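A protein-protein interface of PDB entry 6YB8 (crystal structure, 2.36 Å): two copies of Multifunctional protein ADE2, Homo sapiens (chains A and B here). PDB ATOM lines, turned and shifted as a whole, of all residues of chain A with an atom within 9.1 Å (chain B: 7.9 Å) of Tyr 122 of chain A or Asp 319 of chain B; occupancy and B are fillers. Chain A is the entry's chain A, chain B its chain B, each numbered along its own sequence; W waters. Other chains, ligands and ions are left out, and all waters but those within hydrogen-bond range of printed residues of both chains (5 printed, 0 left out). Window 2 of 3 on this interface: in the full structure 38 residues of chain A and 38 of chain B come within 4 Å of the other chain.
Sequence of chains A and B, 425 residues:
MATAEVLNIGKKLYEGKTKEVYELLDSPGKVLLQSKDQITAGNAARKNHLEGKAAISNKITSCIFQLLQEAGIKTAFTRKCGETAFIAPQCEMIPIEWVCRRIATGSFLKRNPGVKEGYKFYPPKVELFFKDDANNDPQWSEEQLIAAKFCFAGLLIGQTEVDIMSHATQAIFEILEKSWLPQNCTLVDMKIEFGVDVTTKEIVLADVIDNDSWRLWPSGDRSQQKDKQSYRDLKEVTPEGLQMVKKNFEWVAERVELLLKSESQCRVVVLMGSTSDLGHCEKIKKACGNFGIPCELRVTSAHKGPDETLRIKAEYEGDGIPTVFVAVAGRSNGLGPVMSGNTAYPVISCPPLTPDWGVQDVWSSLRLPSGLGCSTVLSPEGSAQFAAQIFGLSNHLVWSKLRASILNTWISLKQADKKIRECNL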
ATOM      1  N   ARG A 101      28.519   9.278  10.287  1.00  0.00           N
ATOM      2  CA  ARG A 101      27.845   9.310  11.611  1.00  0.00           C
ATOM      3  C   ARG A 101      27.889   7.931  12.240  1.00  0.00           C
ATOM      4  O   ARG A 101      27.526   6.966  11.560  1.00  0.00           O
ATOM      5  CB  ARG A 101      26.383   9.753  11.463  1.00  0.00           C
ATOM      6  CG  ARG A 101      26.192  11.075  10.731  1.00  0.00           C
ATOM      7  CD  ARG A 101      24.729  11.381  10.446  1.00  0.00           C
ATOM      8  NE  ARG A 101      24.606  12.511   9.562  1.00  0.00           N
ATOM      9  CZ  ARG A 101      24.676  13.787   9.948  1.00  0.00           C
ATOM     10  NH1 ARG A 101      24.873  14.096  11.221  1.00  0.00           N
ATOM     11  NH2 ARG A 101      24.612  14.761   9.043  1.00  0.00           N
ATOM     12  N   ARG A 102      28.245   7.865  13.517  1.00  0.00           N
ATOM     13  CA  ARG A 102      27.912   6.712  14.390  1.00  0.00           C
ATOM     14  C   ARG A 102      26.573   6.932  15.099  1.00  0.00           C
ATOM     15  O   ARG A 102      25.817   5.977  15.258  1.00  0.00           O
ATOM     16  CB  ARG A 102      29.005   6.479  15.432  1.00  0.00           C
ATOM     17  CG  ARG A 102      28.691   5.311  16.347  1.00  0.00           C
ATOM     18  CD  ARG A 102      28.644   4.032  15.545  1.00  0.00           C
ATOM     19  NE  ARG A 102      29.985   3.624  15.149  1.00  0.00           N
ATOM     20  CZ  ARG A 102      30.266   2.563  14.442  1.00  0.00           C
ATOM     21  NH1 ARG A 102      29.306   1.825  13.902  1.00  0.00           N
ATOM     22  NH2 ARG A 102      31.528   2.293  14.194  1.00  0.00           N
ATOM     23  N   ILE A 103      26.305   8.155  15.546  1.00  0.00           N
ATOM     24  CA  ILE A 103      25.129   8.490  16.392  1.00  0.00           C
ATOM     25  C   ILE A 103      24.340   9.568  15.676  1.00  0.00           C
ATOM     26  O   ILE A 103      24.954  10.560  15.317  1.00  0.00           O
ATOM     27  CB  ILE A 103      25.587   8.972  17.767  1.00  0.00           C
ATOM     28  CG1 ILE A 103      26.303   7.868  18.546  1.00  0.00           C
ATOM     29  CG2 ILE A 103      24.393   9.492  18.537  1.00  0.00           C
ATOM     30  CD1 ILE A 103      27.148   8.376  19.684  1.00  0.00           C
ATOM     31  N   ALA A 104      23.039   9.393  15.531  1.00  0.00           N
ATOM     32  CA  ALA A 104      22.187  10.409  14.898  1.00  0.00           C
ATOM     33  C   ALA A 104      22.063  11.594  15.841  1.00  0.00           C
ATOM     34  O   ALA A 104      21.507  11.415  16.914  1.00  0.00           O
ATOM     35  CB  ALA A 104      20.828   9.874  14.555  1.00  0.00           C
ATOM     36  N   GLY A 118      20.573   9.706  19.464  1.00  0.00           N
ATOM     37  CA  GLY A 118      21.226   8.495  20.016  1.00  0.00           C
ATOM     38  C   GLY A 118      21.054   7.245  19.153  1.00  0.00           C
ATOM     39  O   GLY A 118      21.701   6.226  19.455  1.00  0.00           O
ATOM     40  N   TYR A 119      20.243   7.301  18.107  1.00  0.00           N
ATOM     41  CA  TYR A 119      20.119   6.171  17.154  1.00  0.00           C
ATOM     42  C   TYR A 119      21.511   5.804  16.626  1.00  0.00           C
ATOM     43  O   TYR A 119      22.228   6.675  16.168  1.00  0.00           O
ATOM     44  CB  TYR A 119      19.202   6.535  15.988  1.00  0.00           C
ATOM     45  CG  TYR A 119      18.954   5.407  15.020  1.00  0.00           C
ATOM     46  CD1 TYR A 119      19.781   5.203  13.940  1.00  0.00           C
ATOM     47  CD2 TYR A 119      17.877   4.558  15.182  1.00  0.00           C
ATOM     48  CE1 TYR A 119      19.568   4.172  13.053  1.00  0.00           C
ATOM     49  CE2 TYR A 119      17.631   3.523  14.298  1.00  0.00           C
ATOM     50  CZ  TYR A 119      18.477   3.338  13.228  1.00  0.00           C
ATOM     51  OH  TYR A 119      18.204   2.323  12.378  1.00  0.00           O
ATOM     52  N   LYS A 120      21.881   4.542  16.693  1.00  0.00           N
ATOM     53  CA  LYS A 120      23.226   4.078  16.283  1.00  0.00           C
ATOM     54  C   LYS A 120      23.206   3.537  14.847  1.00  0.00           C
ATOM     55  O   LYS A 120      22.294   2.774  14.462  1.00  0.00           O
ATOM     56  CB  LYS A 120      23.726   3.018  17.258  1.00  0.00           C
ATOM     57  CG  LYS A 120      23.893   3.485  18.689  1.00  0.00           C
ATOM     58  CD  LYS A 120      25.185   4.154  18.939  1.00  0.00           C
ATOM     59  CE  LYS A 120      25.262   4.694  20.349  1.00  0.00           C
ATOM     60  NZ  LYS A 120      26.046   3.802  21.231  1.00  0.00           N
ATOM     61  N   PHE A 121      24.207   3.928  14.067  1.00  0.00           N
ATOM     62  CA  PHE A 121      24.394   3.479  12.680  1.00  0.00           C
ATOM     63  C   PHE A 121      25.421   2.344  12.677  1.00  0.00           C
ATOM     64  O   PHE A 121      26.559   2.546  13.110  1.00  0.00           O
ATOM     65  CB  PHE A 121      24.786   4.653  11.802  1.00  0.00           C
ATOM     66  CG  PHE A 121      23.756   5.756  11.687  1.00  0.00           C
ATOM     67  CD1 PHE A 121      22.600   5.602  10.929  1.00  0.00           C
ATOM     68  CD2 PHE A 121      23.991   6.998  12.270  1.00  0.00           C
ATOM     69  CE1 PHE A 121      21.704   6.648  10.790  1.00  0.00           C
ATOM     70  CE2 PHE A 121      23.076   8.039  12.141  1.00  0.00           C
ATOM     71  CZ  PHE A 121      21.950   7.882  11.368  1.00  0.00           C
ATOM     72  N   TYR A 122      24.986   1.174  12.207  1.00  0.00           N
ATOM     73  CA  TYR A 122      25.818  -0.013  11.948  1.00  0.00           C
ATOM     74  C   TYR A 122      25.547  -0.456  10.510  1.00  0.00           C
ATOM     75  O   TYR A 122      24.459  -0.967  10.218  1.00  0.00           O
ATOM     76  CB  TYR A 122      25.493  -1.090  12.991  1.00  0.00           C
ATOM     77  CG  TYR A 122      25.497  -0.720  14.461  1.00  0.00           C
ATOM     78  CD1 TYR A 122      26.661  -0.338  15.108  1.00  0.00           C
ATOM     79  CD2 TYR A 122      24.350  -0.843  15.246  1.00  0.00           C
ATOM     80  CE1 TYR A 122      26.694  -0.033  16.453  1.00  0.00           C
ATOM     81  CE2 TYR A 122      24.363  -0.575  16.606  1.00  0.00           C
ATOM     82  CZ  TYR A 122      25.548  -0.187  17.213  1.00  0.00           C
ATOM     83  OH  TYR A 122      25.602   0.109  18.555  1.00  0.00           O
ATOM     84  N   PRO A 123      26.466  -0.252   9.535  1.00  0.00           N
ATOM     85  CA  PRO A 123      27.745   0.432   9.738  1.00  0.00           C
ATOM     86  C   PRO A 123      27.545   1.949   9.746  1.00  0.00           C
ATOM     87  O   PRO A 123      26.428   2.433   9.625  1.00  0.00           O
ATOM     88  CB  PRO A 123      28.556   0.025   8.496  1.00  0.00           C
ATOM     89  CG  PRO A 123      27.502  -0.095   7.403  1.00  0.00           C
ATOM     90  CD  PRO A 123      26.241  -0.590   8.111  1.00  0.00           C
ATOM     91  N   PRO A 124      28.609   2.740   9.988  1.00  0.00           N
ATOM     92  CA  PRO A 124      28.477   4.185  10.095  1.00  0.00           C
ATOM     93  C   PRO A 124      27.884   4.743   8.800  1.00  0.00           C
ATOM     94  O   PRO A 124      28.236   4.252   7.737  1.00  0.00           O
ATOM     95  CB  PRO A 124      29.922   4.659  10.329  1.00  0.00           C
ATOM     96  CG  PRO A 124      30.606   3.472  10.972  1.00  0.00           C
ATOM     97  CD  PRO A 124      29.981   2.280  10.286  1.00  0.00           C
ATOM     98  N   LYS A 125      26.952   5.693   8.928  1.00  0.00           N
ATOM     99  CA  LYS A 125      26.190   6.274   7.797  1.00  0.00           C
ATOM    100  C   LYS A 125      27.053   7.369   7.155  1.00  0.00           C
ATOM    101  O   LYS A 125      27.658   8.179   7.905  1.00  0.00           O
ATOM    102  CB  LYS A 125      24.845   6.807   8.276  1.00  0.00           C
ATOM    103  CG  LYS A 125      24.011   7.478   7.192  1.00  0.00           C
ATOM    104  CD  LYS A 125      22.647   6.873   7.011  1.00  0.00           C
ATOM    105  CE  LYS A 125      22.054   7.138   5.641  1.00  0.00           C
ATOM    106  NZ  LYS A 125      21.198   6.015   5.207  1.00  0.00           N
ATOM    107  N   GLN A 170      34.181   6.254   5.498  1.00  0.00           N
ATOM    108  CA  GLN A 170      33.751   5.322   6.553  1.00  0.00           C
ATOM    109  C   GLN A 170      34.996   4.820   7.291  1.00  0.00           C
ATOM    110  O   GLN A 170      35.001   4.797   8.514  1.00  0.00           O
ATOM    111  CB  GLN A 170      32.940   4.232   5.871  1.00  0.00           C
ATOM    112  CG  GLN A 170      32.095   3.413   6.815  1.00  0.00           C
ATOM    113  CD  GLN A 170      31.257   2.436   6.029  1.00  0.00           C
ATOM    114  OE1 GLN A 170      31.595   1.260   6.001  1.00  0.00           O
ATOM    115  NE2 GLN A 170      30.247   2.928   5.315  1.00  0.00           N
ATOM    116  N   GLU A 174      36.034   5.411  11.176  1.00  0.00           N
ATOM    117  CA  GLU A 174      36.267   4.230  12.055  1.00  0.00           C
ATOM    118  C   GLU A 174      37.602   4.357  12.799  1.00  0.00           C
ATOM    119  O   GLU A 174      37.634   4.081  14.015  1.00  0.00           O
ATOM    120  CB  GLU A 174      36.223   2.941  11.232  1.00  0.00           C
ATOM    121  CG  GLU A 174      34.814   2.456  10.943  1.00  0.00           C
ATOM    122  CD  GLU A 174      34.731   1.301   9.960  1.00  0.00           C
ATOM    123  OE1 GLU A 174      35.495   0.329  10.124  1.00  0.00           O
ATOM    124  OE2 GLU A 174      33.901   1.376   9.032  1.00  0.00           O
ATOM    125  N   GLU A 177      37.507   7.092  15.286  1.00  0.00           N
ATOM    126  CA  GLU A 177      36.591   6.649  16.377  1.00  0.00           C
ATOM    127  C   GLU A 177      37.381   5.745  17.327  1.00  0.00           C
ATOM    128  O   GLU A 177      37.326   5.935  18.545  1.00  0.00           O
ATOM    129  CB  GLU A 177      35.393   5.936  15.761  1.00  0.00           C
ATOM    130  CG  GLU A 177      34.315   5.519  16.724  1.00  0.00           C
ATOM    131  CD  GLU A 177      33.219   4.681  16.081  1.00  0.00           C
ATOM    132  OE1 GLU A 177      33.598   3.815  15.247  1.00  0.00           O
ATOM    133  OE2 GLU A 177      31.988   4.918  16.391  1.00  0.00           O
ATOM    134  N   LYS A 178      38.097   4.777  16.771  1.00  0.00           N
ATOM    135  CA  LYS A 178      38.869   3.798  17.570  1.00  0.00           C
ATOM    136  C   LYS A 178      39.979   4.527  18.316  1.00  0.00           C
ATOM    137  O   LYS A 178      40.299   4.122  19.430  1.00  0.00           O
ATOM    138  CB  LYS A 178      39.472   2.705  16.687  1.00  0.00           C
ATOM    139  CG  LYS A 178      40.102   1.544  17.465  1.00  0.00           C
ATOM    140  CD  LYS A 178      39.086   0.568  18.046  1.00  0.00           C
ATOM    141  CE  LYS A 178      38.388  -0.265  16.975  1.00  0.00           C
ATOM    142  NZ  LYS A 178      37.214  -0.962  17.542  1.00  0.00           N
ATOM    143  N   LEU A 181      38.872   6.404  21.505  1.00  0.00           N
ATOM    144  CA  LEU A 181      38.240   5.536  22.533  1.00  0.00           C
ATOM    145  C   LEU A 181      39.102   5.466  23.797  1.00  0.00           C
ATOM    146  O   LEU A 181      38.575   5.573  24.899  1.00  0.00           O
ATOM    147  CB  LEU A 181      37.996   4.139  21.943  1.00  0.00           C
ATOM    148  CG  LEU A 181      36.752   3.396  22.430  1.00  0.00           C
ATOM    149  CD1 LEU A 181      35.508   4.260  22.374  1.00  0.00           C
ATOM    150  CD2 LEU A 181      36.538   2.149  21.590  1.00  0.00           C
ATOM    151  N   GLN B 265      36.660  -5.680  28.177  1.00  0.00           N
ATOM    152  CA  GLN B 265      35.515  -6.505  27.742  1.00  0.00           C
ATOM    153  C   GLN B 265      35.939  -7.456  26.619  1.00  0.00           C
ATOM    154  O   GLN B 265      36.802  -7.122  25.822  1.00  0.00           O
ATOM    155  CB  GLN B 265      34.370  -5.601  27.305  1.00  0.00           C
ATOM    156  CG  GLN B 265      33.712  -4.842  28.444  1.00  0.00           C
ATOM    157  CD  GLN B 265      32.526  -4.081  27.900  1.00  0.00           C
ATOM    158  OE1 GLN B 265      31.383  -4.535  28.007  1.00  0.00           O
ATOM    159  NE2 GLN B 265      32.818  -2.973  27.226  1.00  0.00           N
ATOM    160  N   ARG B 267      34.331 -10.764  23.927  1.00  0.00           N
ATOM    161  CA  ARG B 267      33.136 -11.314  23.290  1.00  0.00           C
ATOM    162  C   ARG B 267      33.565 -12.219  22.134  1.00  0.00           C
ATOM    163  O   ARG B 267      34.402 -11.839  21.342  1.00  0.00           O
ATOM    164  CB  ARG B 267      32.233 -10.169  22.843  1.00  0.00           C
ATOM    165  CG  ARG B 267      30.996 -10.636  22.103  1.00  0.00           C
ATOM    166  CD  ARG B 267      30.095  -9.452  21.874  1.00  0.00           C
ATOM    167  NE  ARG B 267      30.649  -8.497  20.927  1.00  0.00           N
ATOM    168  CZ  ARG B 267      30.127  -7.311  20.677  1.00  0.00           C
ATOM    169  NH1 ARG B 267      29.054  -6.891  21.337  1.00  0.00           N
ATOM    170  NH2 ARG B 267      30.687  -6.525  19.767  1.00  0.00           N
ATOM    171  N   GLU B 296      27.837 -14.955  21.663  1.00  0.00           N
ATOM    172  CA  GLU B 296      26.565 -14.818  20.931  1.00  0.00           C
ATOM    173  C   GLU B 296      26.583 -15.725  19.693  1.00  0.00           C
ATOM    174  O   GLU B 296      27.636 -15.799  19.038  1.00  0.00           O
ATOM    175  CB  GLU B 296      26.405 -13.347  20.568  1.00  0.00           C
ATOM    176  CG  GLU B 296      26.099 -12.516  21.799  1.00  0.00           C
ATOM    177  CD  GLU B 296      25.868 -11.053  21.535  1.00  0.00           C
ATOM    178  OE1 GLU B 296      25.054 -10.725  20.621  1.00  0.00           O
ATOM    179  OE2 GLU B 296      26.497 -10.245  22.259  1.00  0.00           O
ATOM    180  N   LEU B 310      27.554  -8.973   6.239  1.00  0.00           N
ATOM    181  CA  LEU B 310      28.266  -7.698   6.446  1.00  0.00           C
ATOM    182  C   LEU B 310      27.508  -6.786   7.421  1.00  0.00           C
ATOM    183  O   LEU B 310      28.161  -6.179   8.256  1.00  0.00           O
ATOM    184  CB  LEU B 310      28.453  -7.029   5.089  1.00  0.00           C
ATOM    185  CG  LEU B 310      29.272  -7.808   4.067  1.00  0.00           C
ATOM    186  CD1 LEU B 310      29.267  -7.050   2.735  1.00  0.00           C
ATOM    187  CD2 LEU B 310      30.689  -8.025   4.535  1.00  0.00           C
ATOM    188  N   ARG B 311      26.179  -6.727   7.366  1.00  0.00           N
ATOM    189  CA  ARG B 311      25.363  -5.923   8.317  1.00  0.00           C
ATOM    190  C   ARG B 311      25.576  -6.469   9.740  1.00  0.00           C
ATOM    191  O   ARG B 311      25.812  -5.676  10.671  1.00  0.00           O
ATOM    192  CB  ARG B 311      23.905  -5.871   7.872  1.00  0.00           C
ATOM    193  CG  ARG B 311      23.139  -4.644   8.375  1.00  0.00           C
ATOM    194  CD  ARG B 311      21.595  -4.738   8.369  1.00  0.00           C
ATOM    195  NE  ARG B 311      21.146  -5.963   9.050  1.00  0.00           N
ATOM    196  CZ  ARG B 311      21.178  -6.161  10.365  1.00  0.00           C
ATOM    197  NH1 ARG B 311      21.551  -5.181  11.166  1.00  0.00           N
ATOM    198  NH2 ARG B 311      20.806  -7.327  10.886  1.00  0.00           N
ATOM    199  N   ILE B 312      25.615  -7.785   9.913  1.00  0.00           N
ATOM    200  CA  ILE B 312      25.761  -8.393  11.269  1.00  0.00           C
ATOM    201  C   ILE B 312      27.177  -8.112  11.769  1.00  0.00           C
ATOM    202  O   ILE B 312      27.327  -7.695  12.959  1.00  0.00           O
ATOM    203  CB  ILE B 312      25.397  -9.884  11.267  1.00  0.00           C
ATOM    204  CG1 ILE B 312      23.895 -10.041  11.052  1.00  0.00           C
ATOM    205  CG2 ILE B 312      25.842 -10.556  12.542  1.00  0.00           C
ATOM    206  CD1 ILE B 312      23.458 -11.426  10.651  1.00  0.00           C
ATOM    207  N   LYS B 313      28.156  -8.357  10.908  1.00  0.00           N
ATOM    208  CA  LYS B 313      29.573  -8.009  11.186  1.00  0.00           C
ATOM    209  C   LYS B 313      29.608  -6.581  11.727  1.00  0.00           C
ATOM    210  O   LYS B 313      30.201  -6.374  12.794  1.00  0.00           O
ATOM    211  CB  LYS B 313      30.418  -8.171   9.919  1.00  0.00           C
ATOM    212  CG  LYS B 313      31.724  -7.417   9.935  1.00  0.00           C
ATOM    213  CD  LYS B 313      32.478  -7.523   8.635  1.00  0.00           C
ATOM    214  CE  LYS B 313      32.130  -6.409   7.684  1.00  0.00           C
ATOM    215  NZ  LYS B 313      32.639  -5.115   8.176  1.00  0.00           N
ATOM    216  N   ALA B 314      28.947  -5.651  11.042  1.00  0.00           N
ATOM    217  CA  ALA B 314      29.013  -4.207  11.348  1.00  0.00           C
ATOM    218  C   ALA B 314      28.427  -3.914  12.721  1.00  0.00           C
ATOM    219  O   ALA B 314      28.930  -3.011  13.349  1.00  0.00           O
ATOM    220  CB  ALA B 314      28.317  -3.391  10.282  1.00  0.00           C
ATOM    221  N   GLU B 315      27.379  -4.609  13.141  1.00  0.00           N
ATOM    222  CA  GLU B 315      26.758  -4.387  14.470  1.00  0.00           C
ATOM    223  C   GLU B 315      27.790  -4.661  15.562  1.00  0.00           C
ATOM    224  O   GLU B 315      27.758  -3.991  16.584  1.00  0.00           O
ATOM    225  CB  GLU B 315      25.594  -5.331  14.772  1.00  0.00           C
ATOM    226  CG  GLU B 315      24.360  -5.143  13.914  1.00  0.00           C
ATOM    227  CD  GLU B 315      23.224  -6.117  14.237  1.00  0.00           C
ATOM    228  OE1 GLU B 315      23.450  -7.115  14.938  1.00  0.00           O
ATOM    229  OE2 GLU B 315      22.102  -5.864  13.799  1.00  0.00           O
ATOM    230  N   TYR B 316      28.601  -5.695  15.408  1.00  0.00           N
ATOM    231  CA  TYR B 316      29.589  -6.128  16.431  1.00  0.00           C
ATOM    232  C   TYR B 316      30.892  -5.342  16.299  1.00  0.00           C
ATOM    233  O   TYR B 316      31.562  -5.178  17.298  1.00  0.00           O
ATOM    234  CB  TYR B 316      29.812  -7.617  16.277  1.00  0.00           C
ATOM    235  CG  TYR B 316      28.620  -8.419  16.701  1.00  0.00           C
ATOM    236  CD1 TYR B 316      28.200  -8.425  18.023  1.00  0.00           C
ATOM    237  CD2 TYR B 316      27.950  -9.214  15.792  1.00  0.00           C
ATOM    238  CE1 TYR B 316      27.121  -9.190  18.426  1.00  0.00           C
ATOM    239  CE2 TYR B 316      26.868  -9.972  16.175  1.00  0.00           C
ATOM    240  CZ  TYR B 316      26.454  -9.961  17.487  1.00  0.00           C
ATOM    241  OH  TYR B 316      25.401 -10.736  17.827  1.00  0.00           O
ATOM    242  N   GLU B 317      31.221  -4.853  15.108  1.00  0.00           N
ATOM    243  CA  GLU B 317      32.391  -3.956  14.917  1.00  0.00           C
ATOM    244  C   GLU B 317      32.164  -2.603  15.584  1.00  0.00           C
ATOM    245  O   GLU B 317      33.186  -1.961  15.974  1.00  0.00           O
ATOM    246  CB  GLU B 317      32.666  -3.686  13.432  1.00  0.00           C
ATOM    247  CG  GLU B 317      33.367  -4.837  12.735  1.00  0.00           C
ATOM    248  CD  GLU B 317      33.464  -4.646  11.245  1.00  0.00           C
ATOM    249  OE1 GLU B 317      34.482  -5.090  10.665  1.00  0.00           O
ATOM    250  OE2 GLU B 317      32.549  -3.962  10.705  1.00  0.00           O
ATOM    251  N   GLY B 318      30.897  -2.188  15.679  1.00  0.00           N
ATOM    252  CA  GLY B 318      30.486  -0.783  15.818  1.00  0.00           C
ATOM    253  C   GLY B 318      30.191  -0.365  17.238  1.00  0.00           C
ATOM    254  O   GLY B 318      30.068   0.821  17.426  1.00  0.00           O
ATOM    255  N   ASP B 319      30.089  -1.283  18.202  1.00  0.00           N
ATOM    256  CA  ASP B 319      29.631  -0.976  19.587  1.00  0.00           C
ATOM    257  C   ASP B 319      30.793  -0.892  20.579  1.00  0.00           C
ATOM    258  O   ASP B 319      30.498  -0.790  21.767  1.00  0.00           O
ATOM    259  CB  ASP B 319      28.600  -1.994  20.067  1.00  0.00           C
ATOM    260  CG  ASP B 319      29.119  -3.408  20.275  1.00  0.00           C
ATOM    261  OD1 ASP B 319      30.303  -3.666  19.957  1.00  0.00           O
ATOM    262  OD2 ASP B 319      28.345  -4.238  20.788  1.00  0.00           O
ATOM    263  N   GLY B 320      32.045  -1.005  20.136  1.00  0.00           N
ATOM    264  CA  GLY B 320      33.226  -0.807  20.998  1.00  0.00           C
ATOM    265  C   GLY B 320      33.671  -2.044  21.752  1.00  0.00           C
ATOM    266  O   GLY B 320      34.735  -2.009  22.373  1.00  0.00           O
ATOM    267  N   ILE B 321      32.914  -3.112  21.751  1.00  0.00           N
ATOM    268  CA  ILE B 321      33.335  -4.330  22.509  1.00  0.00           C
ATOM    269  C   ILE B 321      34.298  -5.194  21.691  1.00  0.00           C
ATOM    270  O   ILE B 321      33.956  -5.712  20.637  1.00  0.00           O
ATOM    271  CB  ILE B 321      32.110  -5.104  22.965  1.00  0.00           C
ATOM    272  CG1 ILE B 321      31.291  -4.234  23.915  1.00  0.00           C
ATOM    273  CG2 ILE B 321      32.519  -6.412  23.601  1.00  0.00           C
ATOM    274  CD1 ILE B 321      29.918  -4.771  24.159  1.00  0.00           C
ATOM    275  N   PRO B 322      35.537  -5.387  22.178  1.00  0.00           N
ATOM    276  CA  PRO B 322      36.496  -6.239  21.505  1.00  0.00           C
ATOM    277  C   PRO B 322      35.885  -7.625  21.259  1.00  0.00           C
ATOM    278  O   PRO B 322      35.317  -8.209  22.192  1.00  0.00           O
ATOM    279  CB  PRO B 322      37.684  -6.282  22.477  1.00  0.00           C
ATOM    280  CG  PRO B 322      37.608  -5.000  23.217  1.00  0.00           C
ATOM    281  CD  PRO B 322      36.117  -4.776  23.373  1.00  0.00           C
ATOM    282  N   THR B 323      36.061  -8.122  20.036  1.00  0.00           N
ATOM    283  CA  THR B 323      35.324  -9.292  19.525  1.00  0.00           C
ATOM    284  C   THR B 323      36.202 -10.220  18.669  1.00  0.00           C
ATOM    285  O   THR B 323      36.920  -9.731  17.745  1.00  0.00           O
ATOM    286  CB  THR B 323      34.130  -8.823  18.677  1.00  0.00           C
ATOM    287  OG1 THR B 323      33.257  -8.034  19.481  1.00  0.00           O
ATOM    288  CG2 THR B 323      33.369 -10.000  18.140  1.00  0.00           C
ATOM    289  N   TYR B 345      39.111  -7.349  12.982  1.00  0.00           N
ATOM    290  CA  TYR B 345      39.059  -8.255  14.158  1.00  0.00           C
ATOM    291  C   TYR B 345      39.442  -9.662  13.708  1.00  0.00           C
ATOM    292  O   TYR B 345      39.220 -10.061  12.564  1.00  0.00           O
ATOM    293  CB  TYR B 345      37.665  -8.262  14.813  1.00  0.00           C
ATOM    294  CG  TYR B 345      37.255  -7.055  15.611  1.00  0.00           C
ATOM    295  CD1 TYR B 345      38.169  -6.163  16.139  1.00  0.00           C
ATOM    296  CD2 TYR B 345      35.930  -6.831  15.887  1.00  0.00           C
ATOM    297  CE1 TYR B 345      37.768  -5.092  16.910  1.00  0.00           C
ATOM    298  CE2 TYR B 345      35.510  -5.782  16.687  1.00  0.00           C
ATOM    299  CZ  TYR B 345      36.437  -4.911  17.218  1.00  0.00           C
ATOM    300  OH  TYR B 345      36.014  -3.837  17.969  1.00  0.00           O
HETATM  301  O   HOH W   1      35.723  -2.196  15.149  1.00  0.00           O
HETATM  302  O   HOH W   2      34.718  -2.194   9.838  1.00  0.00           O
HETATM  303  O   HOH W   3      29.579  -0.631  12.354  1.00  0.00           O
HETATM  304  O   HOH W   4      37.120  -1.958  20.580  1.00  0.00           O
HETATM  305  O   HOH W   5      22.139  -2.189  10.580  1.00  0.00           O
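Among the printed residues, pairs that only touch across the chains: Arg 102 of chain A with Gly 318 of chain B, Tyr 122 of chain A with Ala 314 of chain B, Tyr 122 of chain A with Glu 315 of chain B, Tyr 122 of chain A with Gly 318 of chain B, Tyr 122 of chain A with Asp 319 of chain B and Pro 123 of chain A with Ala 314 of chain B.
Of the 18 printed residues of chain B, 5 touch a printed residue of chain A. Hydrophobic or aromatic side chains of chain B within 4 Å of the printed part of chain A: Ala 314 and Tyr 345. Of the 17 printed residues of chain A, 4 touch a printed residue of chain B. Printed residues of chain A that touch a printed residue of chain B: Arg 102, Tyr 122, Pro 123 and Lys 178. Hydrophobic or aromatic side chains of chain A that line the printed part of chain B: Tyr 122 and Pro 123. Along chain A the printed residues that touch a printed residue of chain B span positions 102 to 178. Among the printed residues, 7 pairs touch across the chains. Among the printed residues, no Asp or Glu carboxylate lies within 4 Å of a Lys or Arg side-chain nitrogen of the other chain.
Of chain B, only Ala 314 (3.9 Å), Glu 315 (3.8 Å), Gly 318 (3.6 Å) and Asp 319 (3.96 Å) come within 4 Å of Tyr 122 of chain A. Of the printed residues of chain B, Lys 178 of chain A touches Tyr 345. Of the printed residues of chain A, Ala 314 of chain B touches Tyr 122 (3.9 Å) and Pro 123 (3.7 Å). Printed residues of chain A within 4 Å of Glu 315 of chain B: Tyr 122 (3.8 Å). Gly 318 of chain B touches two residues of chain A. Asp 319 of chain B touches just one residue of chain A: Tyr 122. No residue of chain A comes within 4 Å of Gly 320 of chain B. Printed residues of chain A within 4 Å of Tyr 345 of chain B: Lys 178. The nearest residue of chain B that does not touch Tyr 122 of chain A is Arg 311 of chain B (4.3 Å).
No position is printed for both chains.
NZ of Lys 178 of chain A is in hydrogen-bond range of OH of Tyr 345 of chain B (3.1 Å).
Water W4 lies within hydrogen-bond range of the backbone carbonyl oxygen of Gly 320 of chain B, the side-chain amino group of Lys 178 of chain A and the side-chain hydroxyl of Tyr 345 of chain B.
N of Phe 121 of chain A lies within hydrogen-bond range of O of Arg 102 of chain A (2.9 Å). The guanidinium group (NE) of Arg 102 of chain A is in salt-bridge range of the side-chain carboxylate (OE2) of Glu 177 of chain A (2.7 Å). OD2 of Asp 319 of chain B lies within salt-bridge range of NH1 of Arg 267 of chain B.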
